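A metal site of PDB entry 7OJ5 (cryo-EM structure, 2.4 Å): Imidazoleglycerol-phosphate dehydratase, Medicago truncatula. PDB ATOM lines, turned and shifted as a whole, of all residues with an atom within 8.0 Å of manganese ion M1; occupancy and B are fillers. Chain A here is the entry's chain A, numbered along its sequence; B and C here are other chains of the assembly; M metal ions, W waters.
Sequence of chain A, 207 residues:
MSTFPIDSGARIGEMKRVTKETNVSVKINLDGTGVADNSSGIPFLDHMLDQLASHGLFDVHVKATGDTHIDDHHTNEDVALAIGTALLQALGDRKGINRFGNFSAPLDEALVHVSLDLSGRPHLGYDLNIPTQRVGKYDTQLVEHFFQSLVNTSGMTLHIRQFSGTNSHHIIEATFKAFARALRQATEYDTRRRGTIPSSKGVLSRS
The side-chain hydroxyl of Ser 149 sits at hydrogen-bond distance from the backbone carbonyl oxygen of His 145, 3.4 Å away. The backbone NH of His 170 of chain B is in hydrogen-bond range of the side-chain amide oxygen of Asn 167 of chain B, at 3.0 Å. ND1 of His 170 of chain B lies within hydrogen-bond range of OE1 of Glu 109 of chain B.
The nearest printed residue that does not touch manganese ion M1 is Asp 108 of chain B (4.7 Å).
Manganese ion M1 is bound by the side-chain carboxylate (OE1) of Glu 77 (2.3 Å), a ring nitrogen (NE2) of His 145 (2.3 Å), a ring nitrogen (NE2) of His 73 (2.3 Å), a ring nitrogen (NE2) of His 170 of chain B (2.3 Å) and water W1 (2.5 Å).
Water W1 bridges the side-chain carboxylate (OD2) of Asp 108 of chain B (2.7 Å) and the side-chain carboxylate (OE2) of Glu 77 (2.8 Å).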
ATOM      1  N   HIS A  73      -6.696   3.838   2.431  1.00  0.00           N
ATOM      2  CA  HIS A  73      -6.738   3.099   1.168  1.00  0.00           C
ATOM      3  C   HIS A  73      -7.730   3.701   0.187  1.00  0.00           C
ATOM      4  O   HIS A  73      -7.396   3.937  -0.976  1.00  0.00           O
ATOM      5  CB  HIS A  73      -7.073   1.626   1.456  1.00  0.00           C
ATOM      6  CG  HIS A  73      -7.064   0.755   0.239  1.00  0.00           C
ATOM      7  ND1 HIS A  73      -6.092  -0.192   0.004  1.00  0.00           N
ATOM      8  CD2 HIS A  73      -7.921   0.660  -0.808  1.00  0.00           C
ATOM      9  CE1 HIS A  73      -6.339  -0.810  -1.132  1.00  0.00           C
ATOM     10  NE2 HIS A  73      -7.447  -0.316  -1.637  1.00  0.00           N
ATOM     11  N   HIS A  74      -8.963   3.945   0.644  1.00  0.00           N
ATOM     12  CA  HIS A  74     -10.011   4.384  -0.278  1.00  0.00           C
ATOM     13  C   HIS A  74      -9.747   5.806  -0.786  1.00  0.00           C
ATOM     14  O   HIS A  74     -10.036   6.117  -1.943  1.00  0.00           O
ATOM     15  CB  HIS A  74     -11.383   4.289   0.384  1.00  0.00           C
ATOM     16  CG  HIS A  74     -11.776   2.880   0.754  1.00  0.00           C
ATOM     17  ND1 HIS A  74     -12.368   2.578   1.964  1.00  0.00           N
ATOM     18  CD2 HIS A  74     -11.664   1.719   0.082  1.00  0.00           C
ATOM     19  CE1 HIS A  74     -12.601   1.271   2.016  1.00  0.00           C
ATOM     20  NE2 HIS A  74     -12.184   0.722   0.886  1.00  0.00           N
ATOM     21  N   ASN A  76      -6.654   7.223  -1.056  1.00  0.00           N
ATOM     22  CA  ASN A  76      -5.484   7.153  -1.926  1.00  0.00           C
ATOM     23  C   ASN A  76      -5.853   6.636  -3.313  1.00  0.00           C
ATOM     24  O   ASN A  76      -5.338   7.130  -4.323  1.00  0.00           O
ATOM     25  CB  ASN A  76      -4.408   6.285  -1.282  1.00  0.00           C
ATOM     26  CG  ASN A  76      -3.159   6.148  -2.144  1.00  0.00           C
ATOM     27  OD1 ASN A  76      -2.314   7.035  -2.169  1.00  0.00           O
ATOM     28  ND2 ASN A  76      -3.054   5.026  -2.851  1.00  0.00           N
ATOM     29  N   GLU A  77      -6.727   5.640  -3.379  1.00  0.00           N
ATOM     30  CA  GLU A  77      -7.111   5.058  -4.657  1.00  0.00           C
ATOM     31  C   GLU A  77      -7.927   6.040  -5.497  1.00  0.00           C
ATOM     32  O   GLU A  77      -7.727   6.141  -6.718  1.00  0.00           O
ATOM     33  CB  GLU A  77      -7.891   3.759  -4.433  1.00  0.00           C
ATOM     34  CG  GLU A  77      -8.394   3.097  -5.699  1.00  0.00           C
ATOM     35  CD  GLU A  77      -8.820   1.649  -5.487  1.00  0.00           C
ATOM     36  OE1 GLU A  77      -8.674   1.135  -4.347  1.00  0.00           O
ATOM     37  OE2 GLU A  77      -9.313   1.031  -6.450  1.00  0.00           O
ATOM     38  N   ASP A  78      -8.843   6.781  -4.873  1.00  0.00           N
ATOM     39  CA  ASP A  78      -9.710   7.669  -5.625  1.00  0.00           C
ATOM     40  C   ASP A  78      -8.986   8.902  -6.145  1.00  0.00           C
ATOM     41  O   ASP A  78      -9.332   9.419  -7.211  1.00  0.00           O
ATOM     42  CB  ASP A  78     -10.908   8.087  -4.768  1.00  0.00           C
ATOM     43  CG  ASP A  78     -11.919   6.978  -4.596  1.00  0.00           C
ATOM     44  OD1 ASP A  78     -12.121   6.209  -5.552  1.00  0.00           O
ATOM     45  OD2 ASP A  78     -12.509   6.864  -3.493  1.00  0.00           O
ATOM     46  N   LEU A 142       0.757   1.576  -0.317  1.00  0.00           N
ATOM     47  CA  LEU A 142      -0.070   2.431  -1.160  1.00  0.00           C
ATOM     48  C   LEU A 142       0.719   3.123  -2.272  1.00  0.00           C
ATOM     49  O   LEU A 142       0.106   3.747  -3.139  1.00  0.00           O
ATOM     50  CB  LEU A 142      -0.769   3.482  -0.302  1.00  0.00           C
ATOM     51  CG  LEU A 142      -1.677   2.955   0.813  1.00  0.00           C
ATOM     52  CD1 LEU A 142      -2.274   4.114   1.604  1.00  0.00           C
ATOM     53  CD2 LEU A 142      -2.772   2.074   0.243  1.00  0.00           C
ATOM     54  N   HIS A 145      -0.127   1.026  -5.241  1.00  0.00           N
ATOM     55  CA  HIS A 145      -1.541   1.199  -5.581  1.00  0.00           C
ATOM     56  C   HIS A 145      -1.814   2.549  -6.223  1.00  0.00           C
ATOM     57  O   HIS A 145      -2.720   2.669  -7.048  1.00  0.00           O
ATOM     58  CB  HIS A 145      -2.395   1.018  -4.329  1.00  0.00           C
ATOM     59  CG  HIS A 145      -3.797   0.569  -4.610  1.00  0.00           C
ATOM     60  ND1 HIS A 145      -4.551   1.089  -5.638  1.00  0.00           N
ATOM     61  CD2 HIS A 145      -4.583  -0.343  -3.990  1.00  0.00           C
ATOM     62  CE1 HIS A 145      -5.744   0.518  -5.634  1.00  0.00           C
ATOM     63  NE2 HIS A 145      -5.787  -0.352  -4.647  1.00  0.00           N
ATOM     64  N   SER A 149      -3.300   2.728 -10.250  1.00  0.00           N
ATOM     65  CA  SER A 149      -4.573   3.368 -10.565  1.00  0.00           C
ATOM     66  C   SER A 149      -4.394   4.528 -11.529  1.00  0.00           C
ATOM     67  O   SER A 149      -5.324   4.872 -12.276  1.00  0.00           O
ATOM     68  CB  SER A 149      -5.260   3.843  -9.285  1.00  0.00           C
ATOM     69  OG  SER A 149      -5.787   2.753  -8.546  1.00  0.00           O
ATOM     70  N   LEU B 107     -10.356 -10.044  -6.261  1.00  0.00           N
ATOM     71  CA  LEU B 107     -10.313  -8.605  -5.946  1.00  0.00           C
ATOM     72  C   LEU B 107      -8.932  -8.102  -6.396  1.00  0.00           C
ATOM     73  O   LEU B 107      -7.961  -8.187  -5.653  1.00  0.00           O
ATOM     74  CB  LEU B 107     -10.559  -8.344  -4.471  1.00  0.00           C
ATOM     75  CG  LEU B 107     -11.304  -7.069  -4.050  1.00  0.00           C
ATOM     76  CD1 LEU B 107     -11.487  -7.033  -2.539  1.00  0.00           C
ATOM     77  CD2 LEU B 107     -10.616  -5.799  -4.537  1.00  0.00           C
ATOM     78  N   ASP B 108      -8.890  -7.567  -7.622  1.00  0.00           N
ATOM     79  CA  ASP B 108      -7.659  -7.093  -8.262  1.00  0.00           C
ATOM     80  C   ASP B 108      -6.682  -8.272  -8.321  1.00  0.00           C
ATOM     81  O   ASP B 108      -6.998  -9.267  -8.988  1.00  0.00           O
ATOM     82  CB  ASP B 108      -7.157  -5.839  -7.544  1.00  0.00           C
ATOM     83  CG  ASP B 108      -7.964  -4.607  -7.905  1.00  0.00           C
ATOM     84  OD1 ASP B 108      -9.111  -4.748  -8.374  1.00  0.00           O
ATOM     85  OD2 ASP B 108      -7.447  -3.478  -7.716  1.00  0.00           O
ATOM     86  N   GLU B 109      -5.529  -8.206  -7.665  1.00  0.00           N
ATOM     87  CA  GLU B 109      -4.560  -9.292  -7.706  1.00  0.00           C
ATOM     88  C   GLU B 109      -4.855 -10.404  -6.713  1.00  0.00           C
ATOM     89  O   GLU B 109      -4.195 -11.451  -6.780  1.00  0.00           O
ATOM     90  CB  GLU B 109      -3.153  -8.726  -7.466  1.00  0.00           C
ATOM     91  CG  GLU B 109      -2.717  -8.668  -6.000  1.00  0.00           C
ATOM     92  CD  GLU B 109      -3.522  -7.671  -5.189  1.00  0.00           C
ATOM     93  OE1 GLU B 109      -3.971  -6.651  -5.752  1.00  0.00           O
ATOM     94  OE2 GLU B 109      -3.699  -7.909  -3.978  1.00  0.00           O
ATOM     95  N   ASN B 167      -1.729  -7.088  -1.543  1.00  0.00           N
ATOM     96  CA  ASN B 167      -2.216  -5.994  -0.724  1.00  0.00           C
ATOM     97  C   ASN B 167      -3.041  -6.530   0.450  1.00  0.00           C
ATOM     98  O   ASN B 167      -3.912  -7.388   0.269  1.00  0.00           O
ATOM     99  CB  ASN B 167      -3.052  -5.037  -1.570  1.00  0.00           C
ATOM    100  CG  ASN B 167      -3.511  -3.813  -0.812  1.00  0.00           C
ATOM    101  OD1 ASN B 167      -4.525  -3.846  -0.121  1.00  0.00           O
ATOM    102  ND2 ASN B 167      -2.750  -2.729  -0.926  1.00  0.00           N
ATOM    103  N   HIS B 169      -5.275  -4.981   2.448  1.00  0.00           N
ATOM    104  CA  HIS B 169      -6.685  -4.613   2.393  1.00  0.00           C
ATOM    105  C   HIS B 169      -7.453  -5.489   1.411  1.00  0.00           C
ATOM    106  O   HIS B 169      -8.577  -5.908   1.695  1.00  0.00           O
ATOM    107  CB  HIS B 169      -6.827  -3.133   2.031  1.00  0.00           C
ATOM    108  CG  HIS B 169      -8.212  -2.589   2.146  1.00  0.00           C
ATOM    109  ND1 HIS B 169      -8.562  -1.622   3.071  1.00  0.00           N
ATOM    110  CD2 HIS B 169      -9.345  -2.861   1.450  1.00  0.00           C
ATOM    111  CE1 HIS B 169      -9.841  -1.334   2.941  1.00  0.00           C
ATOM    112  NE2 HIS B 169     -10.336  -2.066   1.962  1.00  0.00           N
ATOM    113  N   HIS B 170      -6.859  -5.771   0.248  1.00  0.00           N
ATOM    114  CA  HIS B 170      -7.543  -6.554  -0.771  1.00  0.00           C
ATOM    115  C   HIS B 170      -7.717  -8.010  -0.334  1.00  0.00           C
ATOM    116  O   HIS B 170      -8.752  -8.618  -0.612  1.00  0.00           O
ATOM    117  CB  HIS B 170      -6.780  -6.484  -2.097  1.00  0.00           C
ATOM    118  CG  HIS B 170      -6.838  -5.130  -2.752  1.00  0.00           C
ATOM    119  ND1 HIS B 170      -6.096  -4.819  -3.865  1.00  0.00           N
ATOM    120  CD2 HIS B 170      -7.552  -4.027  -2.449  1.00  0.00           C
ATOM    121  CE1 HIS B 170      -6.346  -3.570  -4.220  1.00  0.00           C
ATOM    122  NE2 HIS B 170      -7.231  -3.074  -3.378  1.00  0.00           N
ATOM    123  N   GLU B 173     -10.522  -8.290   2.560  1.00  0.00           N
ATOM    124  CA  GLU B 173     -11.868  -7.911   2.151  1.00  0.00           C
ATOM    125  C   GLU B 173     -12.365  -8.807   1.015  1.00  0.00           C
ATOM    126  O   GLU B 173     -13.575  -8.935   0.802  1.00  0.00           O
ATOM    127  CB  GLU B 173     -11.880  -6.413   1.809  1.00  0.00           C
ATOM    128  CG  GLU B 173     -13.031  -5.844   1.011  1.00  0.00           C
ATOM    129  CD  GLU B 173     -12.917  -4.324   0.891  1.00  0.00           C
ATOM    130  OE1 GLU B 173     -13.055  -3.651   1.940  1.00  0.00           O
ATOM    131  OE2 GLU B 173     -12.695  -3.787  -0.208  1.00  0.00           O
ATOM    132  N   ARG C 121     -12.225  -2.337 -13.082  1.00  0.00           N
ATOM    133  CA  ARG C 121     -10.790  -2.267 -12.850  1.00  0.00           C
ATOM    134  C   ARG C 121     -10.104  -3.390 -13.612  1.00  0.00           C
ATOM    135  O   ARG C 121     -10.325  -4.570 -13.312  1.00  0.00           O
ATOM    136  CB  ARG C 121     -10.470  -2.377 -11.354  1.00  0.00           C
ATOM    137  CG  ARG C 121     -11.048  -1.238 -10.519  1.00  0.00           C
ATOM    138  CD  ARG C 121     -10.726  -1.403  -9.042  1.00  0.00           C
ATOM    139  NE  ARG C 121     -11.255  -2.640  -8.493  1.00  0.00           N
ATOM    140  CZ  ARG C 121     -12.496  -2.800  -8.070  1.00  0.00           C
ATOM    141  NH1 ARG C 121     -13.383  -1.823  -8.117  1.00  0.00           N
ATOM    142  NH2 ARG C 121     -12.868  -3.987  -7.577  1.00  0.00           N
HETATM  143 MN    MN M   1      -7.829  -0.894  -3.832  1.00  0.00          MN
HETATM  144 MN    MN M   2     -12.521  -1.693   1.159  1.00  0.00          MN
HETATM  145  O   HOH W   1      -8.598  -1.675  -6.029  1.00  0.00           O
